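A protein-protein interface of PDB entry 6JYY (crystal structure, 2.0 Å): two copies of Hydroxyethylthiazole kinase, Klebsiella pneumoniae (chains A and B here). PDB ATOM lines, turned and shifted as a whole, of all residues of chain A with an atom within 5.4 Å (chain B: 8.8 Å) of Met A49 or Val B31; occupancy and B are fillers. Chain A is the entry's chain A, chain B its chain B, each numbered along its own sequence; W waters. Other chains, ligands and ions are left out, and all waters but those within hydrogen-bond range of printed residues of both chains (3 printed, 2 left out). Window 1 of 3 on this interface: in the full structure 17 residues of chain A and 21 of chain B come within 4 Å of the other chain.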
ATOM      1  N   HIS A  25     -21.650   4.199  13.606  1.00  0.00           N
ATOM      2  CA  HIS A  25     -21.246   2.954  12.960  1.00  0.00           C
ATOM      3  C   HIS A  25     -20.345   2.214  13.957  1.00  0.00           C
ATOM      4  O   HIS A  25     -19.210   2.596  14.186  1.00  0.00           O
ATOM      5  CB  HIS A  25     -20.525   3.256  11.620  1.00  0.00           C
ATOM      6  CG  HIS A  25     -20.084   2.047  10.848  1.00  0.00           C
ATOM      7  ND1 HIS A  25     -19.345   2.144   9.688  1.00  0.00           N
ATOM      8  CD2 HIS A  25     -20.258   0.718  11.069  1.00  0.00           C
ATOM      9  CE1 HIS A  25     -19.095   0.934   9.224  1.00  0.00           C
ATOM     10  NE2 HIS A  25     -19.641   0.052  10.041  1.00  0.00           N
ATOM     11  N   CYS A  26     -20.864   1.157  14.552  1.00  0.00           N
ATOM     12  CA  CYS A  26     -20.098   0.429  15.577  1.00  0.00           C
ATOM     13  C   CYS A  26     -19.426  -0.805  14.999  1.00  0.00           C
ATOM     14  O   CYS A  26     -20.103  -1.770  14.614  1.00  0.00           O
ATOM     15  CB  CYS A  26     -20.993   0.020  16.712  1.00  0.00           C
ATOM     16  SG  CYS A  26     -21.791   1.362  17.567  1.00  0.00           S
ATOM     17  N   THR A  28     -17.378  -3.189  16.680  1.00  0.00           N
ATOM     18  CA  THR A  28     -16.948  -3.574  18.025  1.00  0.00           C
ATOM     19  C   THR A  28     -16.854  -5.093  18.214  1.00  0.00           C
ATOM     20  O   THR A  28     -17.255  -5.866  17.345  1.00  0.00           O
ATOM     21  CB  THR A  28     -17.915  -3.034  19.112  1.00  0.00           C
ATOM     22  OG1 THR A  28     -18.434  -1.762  18.728  1.00  0.00           O
ATOM     23  CG2 THR A  28     -17.212  -2.875  20.409  1.00  0.00           C
ATOM     24  N   GLN A  33     -21.360  -6.222  21.847  1.00  0.00           N
ATOM     25  CA  GLN A  33     -22.166  -5.591  20.796  1.00  0.00           C
ATOM     26  C   GLN A  33     -23.609  -5.213  21.189  1.00  0.00           C
ATOM     27  O   GLN A  33     -24.130  -4.111  20.855  1.00  0.00           O
ATOM     28  CB  GLN A  33     -22.192  -6.516  19.598  1.00  0.00           C
ATOM     29  CG  GLN A  33     -21.013  -6.263  18.692  1.00  0.00           C
ATOM     30  CD  GLN A  33     -21.197  -6.905  17.364  1.00  0.00           C
ATOM     31  OE1 GLN A  33     -22.159  -6.603  16.658  1.00  0.00           O
ATOM     32  NE2 GLN A  33     -20.300  -7.822  17.016  1.00  0.00           N
ATOM     33  N   THR A  34     -24.272  -6.112  21.901  1.00  0.00           N
ATOM     34  CA  THR A  34     -25.642  -5.862  22.281  1.00  0.00           C
ATOM     35  C   THR A  34     -25.715  -4.715  23.295  1.00  0.00           C
ATOM     36  O   THR A  34     -26.543  -3.791  23.182  1.00  0.00           O
ATOM     37  CB  THR A  34     -26.293  -7.109  22.869  1.00  0.00           C
ATOM     38  OG1 THR A  34     -26.279  -8.160  21.892  1.00  0.00           O
ATOM     39  CG2 THR A  34     -27.704  -6.850  23.275  1.00  0.00           C
ATOM     40  N   THR A  36     -23.550  -2.362  23.758  1.00  0.00           N
ATOM     41  CA  THR A  36     -23.149  -1.116  23.109  1.00  0.00           C
ATOM     42  C   THR A  36     -24.340  -0.520  22.387  1.00  0.00           C
ATOM     43  O   THR A  36     -24.644   0.687  22.530  1.00  0.00           O
ATOM     44  CB  THR A  36     -21.979  -1.343  22.104  1.00  0.00           C
ATOM     45  OG1 THR A  36     -20.812  -1.708  22.833  1.00  0.00           O
ATOM     46  CG2 THR A  36     -21.671  -0.069  21.294  1.00  0.00           C
ATOM     47  N   ALA A  37     -25.021  -1.362  21.607  1.00  0.00           N
ATOM     48  CA  ALA A  37     -26.224  -0.875  20.908  1.00  0.00           C
ATOM     49  C   ALA A  37     -27.301  -0.352  21.879  1.00  0.00           C
ATOM     50  O   ALA A  37     -27.852   0.719  21.674  1.00  0.00           O
ATOM     51  CB  ALA A  37     -26.786  -1.953  20.037  1.00  0.00           C
ATOM     52  N   PRO A  47     -27.414   3.275  16.879  1.00  0.00           N
ATOM     53  CA  PRO A  47     -26.332   2.345  16.574  1.00  0.00           C
ATOM     54  C   PRO A  47     -26.564   1.604  15.279  1.00  0.00           C
ATOM     55  O   PRO A  47     -27.694   1.265  14.983  1.00  0.00           O
ATOM     56  CB  PRO A  47     -26.380   1.394  17.758  1.00  0.00           C
ATOM     57  CG  PRO A  47     -27.787   1.313  18.049  1.00  0.00           C
ATOM     58  CD  PRO A  47     -28.283   2.727  17.936  1.00  0.00           C
ATOM     59  N   ALA A  48     -25.515   1.352  14.522  1.00  0.00           N
ATOM     60  CA  ALA A  48     -25.628   0.467  13.395  1.00  0.00           C
ATOM     61  C   ALA A  48     -24.378  -0.369  13.360  1.00  0.00           C
ATOM     62  O   ALA A  48     -23.272   0.131  13.557  1.00  0.00           O
ATOM     63  CB  ALA A  48     -25.820   1.249  12.082  1.00  0.00           C
ATOM     64  N   MET A  49     -24.552  -1.659  13.123  1.00  0.00           N
ATOM     65  CA  MET A  49     -23.419  -2.556  13.066  1.00  0.00           C
ATOM     66  C   MET A  49     -23.356  -3.088  11.653  1.00  0.00           C
ATOM     67  O   MET A  49     -24.294  -3.707  11.166  1.00  0.00           O
ATOM     68  CB  MET A  49     -23.558  -3.663  14.107  1.00  0.00           C
ATOM     69  CG  MET A  49     -23.182  -3.254  15.546  1.00  0.00           C
ATOM     70  SD  MET A  49     -24.229  -2.074  16.455  1.00  0.00           S
ATOM     71  CE  MET A  49     -23.372  -2.233  18.052  1.00  0.00           C
ATOM     72  N   VAL A  50     -22.276  -2.756  10.966  1.00  0.00           N
ATOM     73  CA  VAL A  50     -22.086  -3.155   9.577  1.00  0.00           C
ATOM     74  C   VAL A  50     -20.658  -3.647   9.417  1.00  0.00           C
ATOM     75  O   VAL A  50     -19.715  -2.886   9.686  1.00  0.00           O
ATOM     76  CB  VAL A  50     -22.373  -1.959   8.596  1.00  0.00           C
ATOM     77  CG1 VAL A  50     -22.373  -2.416   7.168  1.00  0.00           C
ATOM     78  CG2 VAL A  50     -23.700  -1.322   8.926  1.00  0.00           C
ATOM     79  N   ILE A  51     -20.490  -4.885   8.948  1.00  0.00           N
ATOM     80  CA  ILE A  51     -19.171  -5.535   8.977  1.00  0.00           C
ATOM     81  C   ILE A  51     -18.639  -6.108   7.654  1.00  0.00           C
ATOM     82  O   ILE A  51     -17.454  -6.383   7.547  1.00  0.00           O
ATOM     83  CB  ILE A  51     -19.142  -6.688  10.039  1.00  0.00           C
ATOM     84  CG1 ILE A  51     -20.258  -7.716   9.818  1.00  0.00           C
ATOM     85  CG2 ILE A  51     -19.219  -6.098  11.437  1.00  0.00           C
ATOM     86  CD1 ILE A  51     -20.028  -9.058  10.548  1.00  0.00           C
ATOM     87  N   THR B  28     -29.239 -15.487  12.379  1.00  0.00           N
ATOM     88  CA  THR B  28     -29.565 -14.069  12.576  1.00  0.00           C
ATOM     89  C   THR B  28     -28.311 -13.290  12.887  1.00  0.00           C
ATOM     90  O   THR B  28     -27.207 -13.838  12.891  1.00  0.00           O
ATOM     91  CB  THR B  28     -30.609 -13.843  13.681  1.00  0.00           C
ATOM     92  OG1 THR B  28     -31.084 -12.476  13.641  1.00  0.00           O
ATOM     93  CG2 THR B  28     -30.031 -14.141  15.088  1.00  0.00           C
ATOM     94  N   ASN B  29     -28.471 -11.995  13.120  1.00  0.00           N
ATOM     95  CA  ASN B  29     -27.306 -11.126  13.205  1.00  0.00           C
ATOM     96  C   ASN B  29     -26.657 -11.120  14.593  1.00  0.00           C
ATOM     97  O   ASN B  29     -27.257 -11.477  15.608  1.00  0.00           O
ATOM     98  CB  ASN B  29     -27.672  -9.701  12.761  1.00  0.00           C
ATOM     99  CG  ASN B  29     -28.571  -8.973  13.746  1.00  0.00           C
ATOM    100  OD1 ASN B  29     -28.147  -8.558  14.833  1.00  0.00           O
ATOM    101  ND2 ASN B  29     -29.791  -8.732  13.334  1.00  0.00           N
ATOM    102  N   ASP B  30     -25.390 -10.750  14.576  1.00  0.00           N
ATOM    103  CA  ASP B  30     -24.523 -10.617  15.757  1.00  0.00           C
ATOM    104  C   ASP B  30     -25.096  -9.913  16.960  1.00  0.00           C
ATOM    105  O   ASP B  30     -24.796 -10.271  18.088  1.00  0.00           O
ATOM    106  CB  ASP B  30     -23.255  -9.863  15.349  1.00  0.00           C
ATOM    107  CG  ASP B  30     -22.324 -10.708  14.508  1.00  0.00           C
ATOM    108  OD1 ASP B  30     -22.707 -11.842  14.155  1.00  0.00           O
ATOM    109  OD2 ASP B  30     -21.205 -10.240  14.204  1.00  0.00           O
ATOM    110  N   VAL B  31     -25.936  -8.920  16.737  1.00  0.00           N
ATOM    111  CA  VAL B  31     -26.345  -8.041  17.809  1.00  0.00           C
ATOM    112  C   VAL B  31     -27.540  -8.590  18.602  1.00  0.00           C
ATOM    113  O   VAL B  31     -27.766  -8.190  19.751  1.00  0.00           O
ATOM    114  CB  VAL B  31     -26.676  -6.645  17.224  1.00  0.00           C
ATOM    115  CG1 VAL B  31     -26.894  -5.620  18.311  1.00  0.00           C
ATOM    116  CG2 VAL B  31     -25.509  -6.184  16.338  1.00  0.00           C
ATOM    117  N   VAL B  32     -28.299  -9.496  17.992  1.00  0.00           N
ATOM    118  CA  VAL B  32     -29.590  -9.908  18.554  1.00  0.00           C
ATOM    119  C   VAL B  32     -29.676 -11.392  18.897  1.00  0.00           C
ATOM    120  O   VAL B  32     -30.768 -11.864  19.245  1.00  0.00           O
ATOM    121  CB  VAL B  32     -30.787  -9.576  17.583  1.00  0.00           C
ATOM    122  CG1 VAL B  32     -30.929  -8.089  17.341  1.00  0.00           C
ATOM    123  CG2 VAL B  32     -30.653 -10.337  16.246  1.00  0.00           C
ATOM    124  N   GLN B  33     -28.560 -12.121  18.812  1.00  0.00           N
ATOM    125  CA  GLN B  33     -28.537 -13.581  19.008  1.00  0.00           C
ATOM    126  C   GLN B  33     -29.159 -14.024  20.326  1.00  0.00           C
ATOM    127  O   GLN B  33     -30.100 -14.838  20.391  1.00  0.00           O
ATOM    128  CB  GLN B  33     -27.092 -14.121  18.993  1.00  0.00           C
ATOM    129  CG  GLN B  33     -26.302 -13.931  17.724  1.00  0.00           C
ATOM    130  CD  GLN B  33     -26.342 -15.147  16.839  1.00  0.00           C
ATOM    131  OE1 GLN B  33     -25.979 -16.252  17.258  1.00  0.00           O
ATOM    132  NE2 GLN B  33     -26.786 -14.958  15.600  1.00  0.00           N
ATOM    133  N   THR B  34     -28.616 -13.479  21.397  1.00  0.00           N
ATOM    134  CA  THR B  34     -28.998 -13.909  22.723  1.00  0.00           C
ATOM    135  C   THR B  34     -30.468 -13.620  22.994  1.00  0.00           C
ATOM    136  O   THR B  34     -31.203 -14.468  23.523  1.00  0.00           O
ATOM    137  CB  THR B  34     -28.144 -13.233  23.774  1.00  0.00           C
ATOM    138  OG1 THR B  34     -26.760 -13.399  23.419  1.00  0.00           O
ATOM    139  CG2 THR B  34     -28.424 -13.860  25.131  1.00  0.00           C
ATOM    140  N   PHE B  35     -30.883 -12.409  22.657  1.00  0.00           N
ATOM    141  CA  PHE B  35     -32.267 -11.991  22.916  1.00  0.00           C
ATOM    142  C   PHE B  35     -33.267 -12.790  22.068  1.00  0.00           C
ATOM    143  O   PHE B  35     -34.331 -13.162  22.554  1.00  0.00           O
ATOM    144  CB  PHE B  35     -32.418 -10.497  22.649  1.00  0.00           C
ATOM    145  CG  PHE B  35     -33.782  -9.942  23.007  1.00  0.00           C
ATOM    146  CD1 PHE B  35     -34.245  -9.963  24.311  1.00  0.00           C
ATOM    147  CD2 PHE B  35     -34.583  -9.376  22.028  1.00  0.00           C
ATOM    148  CE1 PHE B  35     -35.484  -9.432  24.626  1.00  0.00           C
ATOM    149  CE2 PHE B  35     -35.825  -8.840  22.339  1.00  0.00           C
ATOM    150  CZ  PHE B  35     -36.270  -8.871  23.633  1.00  0.00           C
ATOM    151  N   THR B  36     -32.940 -13.035  20.801  1.00  0.00           N
ATOM    152  CA  THR B  36     -33.750 -13.919  19.952  1.00  0.00           C
ATOM    153  C   THR B  36     -33.916 -15.299  20.595  1.00  0.00           C
ATOM    154  O   THR B  36     -35.021 -15.841  20.679  1.00  0.00           O
ATOM    155  CB  THR B  36     -33.110 -14.111  18.585  1.00  0.00           C
ATOM    156  OG1 THR B  36     -33.017 -12.851  17.941  1.00  0.00           O
ATOM    157  CG2 THR B  36     -33.922 -15.072  17.718  1.00  0.00           C
ATOM    158  N   ASN B  69     -31.979 -13.764   8.878  1.00  0.00           N
ATOM    159  CA  ASN B  69     -31.910 -12.318   9.166  1.00  0.00           C
ATOM    160  C   ASN B  69     -30.544 -11.835   8.703  1.00  0.00           C
ATOM    161  O   ASN B  69     -29.515 -12.397   9.093  1.00  0.00           O
ATOM    162  CB  ASN B  69     -32.171 -12.039  10.674  1.00  0.00           C
ATOM    163  CG  ASN B  69     -31.858 -10.572  11.111  1.00  0.00           C
ATOM    164  OD1 ASN B  69     -30.760 -10.046  10.889  1.00  0.00           O
ATOM    165  ND2 ASN B  69     -32.813  -9.950  11.783  1.00  0.00           N
ATOM    166  N   VAL B  70     -30.530 -10.832   7.825  1.00  0.00           N
ATOM    167  CA  VAL B  70     -29.294 -10.400   7.144  1.00  0.00           C
ATOM    168  C   VAL B  70     -28.594  -9.175   7.765  1.00  0.00           C
ATOM    169  O   VAL B  70     -27.716  -8.537   7.146  1.00  0.00           O
ATOM    170  CB  VAL B  70     -29.582 -10.075   5.652  1.00  0.00           C
ATOM    171  CG1 VAL B  70     -29.984 -11.324   4.890  1.00  0.00           C
ATOM    172  CG2 VAL B  70     -30.632  -8.985   5.518  1.00  0.00           C
ATOM    173  N   GLY B  71     -28.990  -8.868   8.983  1.00  0.00           N
ATOM    174  CA  GLY B  71     -28.505  -7.728   9.752  1.00  0.00           C
ATOM    175  C   GLY B  71     -27.017  -7.439   9.833  1.00  0.00           C
ATOM    176  O   GLY B  71     -26.626  -6.268   9.867  1.00  0.00           O
ATOM    177  N   THR B  72     -26.182  -8.467   9.913  1.00  0.00           N
ATOM    178  CA  THR B  72     -24.718  -8.267   9.900  1.00  0.00           C
ATOM    179  C   THR B  72     -24.140  -9.243   8.879  1.00  0.00           C
ATOM    180  O   THR B  72     -23.259 -10.060   9.178  1.00  0.00           O
ATOM    181  CB  THR B  72     -24.073  -8.464  11.303  1.00  0.00           C
ATOM    182  OG1 THR B  72     -24.543  -9.682  11.885  1.00  0.00           O
ATOM    183  CG2 THR B  72     -24.438  -7.316  12.230  1.00  0.00           C
ATOM    184  N   LEU B  73     -24.676  -9.155   7.656  1.00  0.00           N
ATOM    185  CA  LEU B  73     -24.332 -10.100   6.604  1.00  0.00           C
ATOM    186  C   LEU B  73     -22.845 -10.064   6.293  1.00  0.00           C
ATOM    187  O   LEU B  73     -22.232  -9.016   6.328  1.00  0.00           O
ATOM    188  CB  LEU B  73     -25.145  -9.801   5.344  1.00  0.00           C
ATOM    189  CG  LEU B  73     -25.093 -10.886   4.260  1.00  0.00           C
ATOM    190  CD1 LEU B  73     -25.901 -12.097   4.689  1.00  0.00           C
ATOM    191  CD2 LEU B  73     -25.583 -10.363   2.928  1.00  0.00           C
ATOM    192  N   VAL B 100     -33.310  -6.927   7.045  1.00  0.00           N
ATOM    193  CA  VAL B 100     -32.735  -5.778   7.741  1.00  0.00           C
ATOM    194  C   VAL B 100     -31.923  -4.866   6.804  1.00  0.00           C
ATOM    195  O   VAL B 100     -30.938  -5.298   6.179  1.00  0.00           O
ATOM    196  CB  VAL B 100     -31.814  -6.238   8.919  1.00  0.00           C
ATOM    197  CG1 VAL B 100     -31.220  -5.029   9.679  1.00  0.00           C
ATOM    198  CG2 VAL B 100     -32.598  -7.067   9.889  1.00  0.00           C
ATOM    199  N   ALA B 101     -32.366  -3.610   6.693  1.00  0.00           N
ATOM    200  CA  ALA B 101     -31.602  -2.556   6.028  1.00  0.00           C
ATOM    201  C   ALA B 101     -31.464  -2.752   4.514  1.00  0.00           C
ATOM    202  O   ALA B 101     -30.551  -2.216   3.886  1.00  0.00           O
ATOM    203  CB  ALA B 101     -30.210  -2.432   6.672  1.00  0.00           C
ATOM    204  N   LEU B 105     -28.377  -0.672   2.029  1.00  0.00           N
ATOM    205  CA  LEU B 105     -27.049  -1.253   1.837  1.00  0.00           C
ATOM    206  C   LEU B 105     -27.098  -2.229   0.669  1.00  0.00           C
ATOM    207  O   LEU B 105     -27.940  -3.114   0.642  1.00  0.00           O
ATOM    208  CB  LEU B 105     -26.567  -1.955   3.117  1.00  0.00           C
ATOM    209  CG  LEU B 105     -26.440  -1.087   4.382  1.00  0.00           C
ATOM    210  CD1 LEU B 105     -26.344  -1.961   5.603  1.00  0.00           C
ATOM    211  CD2 LEU B 105     -25.234  -0.206   4.307  1.00  0.00           C
ATOM    212  N   ARG B 108     -26.334  -6.761   0.718  1.00  0.00           N
ATOM    213  CA  ARG B 108     -27.415  -7.542   1.292  1.00  0.00           C
ATOM    214  C   ARG B 108     -28.717  -7.350   0.502  1.00  0.00           C
ATOM    215  O   ARG B 108     -29.573  -8.241   0.492  1.00  0.00           O
ATOM    216  CB  ARG B 108     -27.614  -7.174   2.766  1.00  0.00           C
ATOM    217  CG  ARG B 108     -28.074  -5.762   3.019  1.00  0.00           C
ATOM    218  CD  ARG B 108     -28.211  -5.517   4.502  1.00  0.00           C
ATOM    219  NE  ARG B 108     -26.912  -5.542   5.180  1.00  0.00           N
ATOM    220  CZ  ARG B 108     -26.737  -5.290   6.475  1.00  0.00           C
ATOM    221  NH1 ARG B 108     -27.778  -5.006   7.250  1.00  0.00           N
ATOM    222  NH2 ARG B 108     -25.515  -5.326   7.005  1.00  0.00           N
ATOM    223  N   VAL B 195     -34.876  -0.316  22.437  1.00  0.00           N
ATOM    224  CA  VAL B 195     -34.277  -1.573  22.849  1.00  0.00           C
ATOM    225  C   VAL B 195     -33.915  -2.276  21.559  1.00  0.00           C
ATOM    226  O   VAL B 195     -34.713  -2.288  20.623  1.00  0.00           O
ATOM    227  CB  VAL B 195     -35.282  -2.419  23.688  1.00  0.00           C
ATOM    228  CG1 VAL B 195     -34.883  -3.887  23.750  1.00  0.00           C
ATOM    229  CG2 VAL B 195     -35.430  -1.829  25.082  1.00  0.00           C
ATOM    230  N   VAL B 196     -32.728  -2.863  21.483  1.00  0.00           N
ATOM    231  CA  VAL B 196     -32.319  -3.477  20.239  1.00  0.00           C
ATOM    232  C   VAL B 196     -32.869  -4.918  20.174  1.00  0.00           C
ATOM    233  O   VAL B 196     -32.972  -5.632  21.188  1.00  0.00           O
ATOM    234  CB  VAL B 196     -30.774  -3.455  20.078  1.00  0.00           C
ATOM    235  CG1 VAL B 196     -30.115  -4.677  20.730  1.00  0.00           C
ATOM    236  CG2 VAL B 196     -30.379  -3.306  18.610  1.00  0.00           C
ATOM    237  N   GLY B 197     -33.252  -5.332  18.976  1.00  0.00           N
ATOM    238  CA  GLY B 197     -33.615  -6.720  18.752  1.00  0.00           C
ATOM    239  C   GLY B 197     -35.097  -7.046  18.741  1.00  0.00           C
ATOM    240  O   GLY B 197     -35.463  -8.125  18.309  1.00  0.00           O
ATOM    241  N   THR B 198     -35.946  -6.143  19.203  1.00  0.00           N
ATOM    242  CA  THR B 198     -37.368  -6.465  19.301  1.00  0.00           C
ATOM    243  C   THR B 198     -37.951  -6.793  17.915  1.00  0.00           C
ATOM    244  O   THR B 198     -38.790  -7.695  17.781  1.00  0.00           O
ATOM    245  CB  THR B 198     -38.152  -5.324  19.950  1.00  0.00           C
ATOM    246  OG1 THR B 198     -37.725  -4.069  19.396  1.00  0.00           O
ATOM    247  CG2 THR B 198     -37.924  -5.334  21.473  1.00  0.00           C
ATOM    248  N   CYS B 200     -36.126  -8.059  15.255  1.00  0.00           N
ATOM    249  CA  CYS B 200     -35.500  -9.280  14.797  1.00  0.00           C
ATOM    250  C   CYS B 200     -36.023 -10.505  15.580  1.00  0.00           C
ATOM    251  O   CYS B 200     -36.078 -11.613  15.049  1.00  0.00           O
ATOM    252  CB  CYS B 200     -33.987  -9.122  14.914  1.00  0.00           C
ATOM    253  SG  CYS B 200     -33.343  -7.654  13.963  1.00  0.00           S
HETATM  254  O   HOH W   1     -26.420 -11.210  21.327  1.00  0.00           O
HETATM  255  O   HOH W   2     -25.361 -10.611  23.723  1.00  0.00           O
HETATM  256  O   HOH W   3     -22.592  -6.389   7.236  1.00  0.00           O
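The side-chain hydroxyl (OG1) of Thr A34 is in hydrogen-bond range of the backbone carbonyl oxygen (O) of Val B31, at 2.6 Å.
Water W3 lies within hydrogen-bond range of the backbone carbonyl oxygen (O) of Leu B73 (2.8 Å), the backbone NH (N) of Ile A51 (3.1 Å) and the guanidinium group (NH2) of Arg B108 (3.1 Å). Water W1 lies within hydrogen-bond range of the side-chain hydroxyl (OG1) of Thr B34 (3.0 Å), the side-chain hydroxyl (OG1) of Thr A34 (3.1 Å) and the backbone NH (N) of Gln B33 (3.4 Å). Water W2 lies within hydrogen-bond range of OG1 of Thr B34 (3.1 Å) and OG1 of Thr A34 (3.2 Å).
Of the 12 printed residues of chain A, 4 touch a printed residue of chain B.
Positions printed for both chains: 28, 33, 34 and 36.
Printed residues of chain B within 4 Å of Gln A33: Asp B30 (3.7 Å) and Val B31 (3.4 Å). Printed residues of chain B within 4 Å of Thr A34: Val B31 (2.6 Å). Ala A48 touches none of the printed residues of chain B. Of chain B, only Val B31 (3.8 Å), Gly B71 (3.7 Å) and Thr B72 (3.8 Å) come within 4 Å of Met A49. Printed residues of chain B within 4 Å of Ile A51: Thr B72. Of the printed residues of chain A, Asp B30 touches Gln A33. Of chain A, only Gln A33, Thr A34 and Met A49 come within 4 Å of Val B31. Gln B33 touches none of the printed residues of chain A. Cys B200 touches none of the printed residues of chain A. The nearest residue of chain B that does not touch Met A49 is Arg B108 (4.6 Å). The nearest residue of chain A that does not touch Val B31 is Ala A37 (4.1 Å). The nearest printed residue of chain B that does not touch Thr A34 is Val B196 (4.1 Å).
Among the printed residues, merely in contact across the chains: Gln A33 with Asp B30 (3.7 Å), Gln A33 with Val B31 (3.4 Å), Met A49 with Val B31 (3.8 Å), Met A49 with Gly B71 (3.7 Å), Met A49 with Thr B72 (3.8 Å) and Ile A51 with Thr B72 (3.6 Å).
The backbone carbonyl oxygen (O) of Gly B71 lies within hydrogen-bond range of the guanidinium group (NH1) of Arg B108, at 3.1 Å. OD1 of Asn B69 lies within hydrogen-bond range of N of Gly B71, 2.9 Å away. The backbone NH (N) of Asp B30 is in hydrogen-bond range of the side-chain hydroxyl (OG1) of Thr B72 (3.0 Å). OD1 of Asn B29 sits at hydrogen-bond distance from N of Val B31 (2.9 Å).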
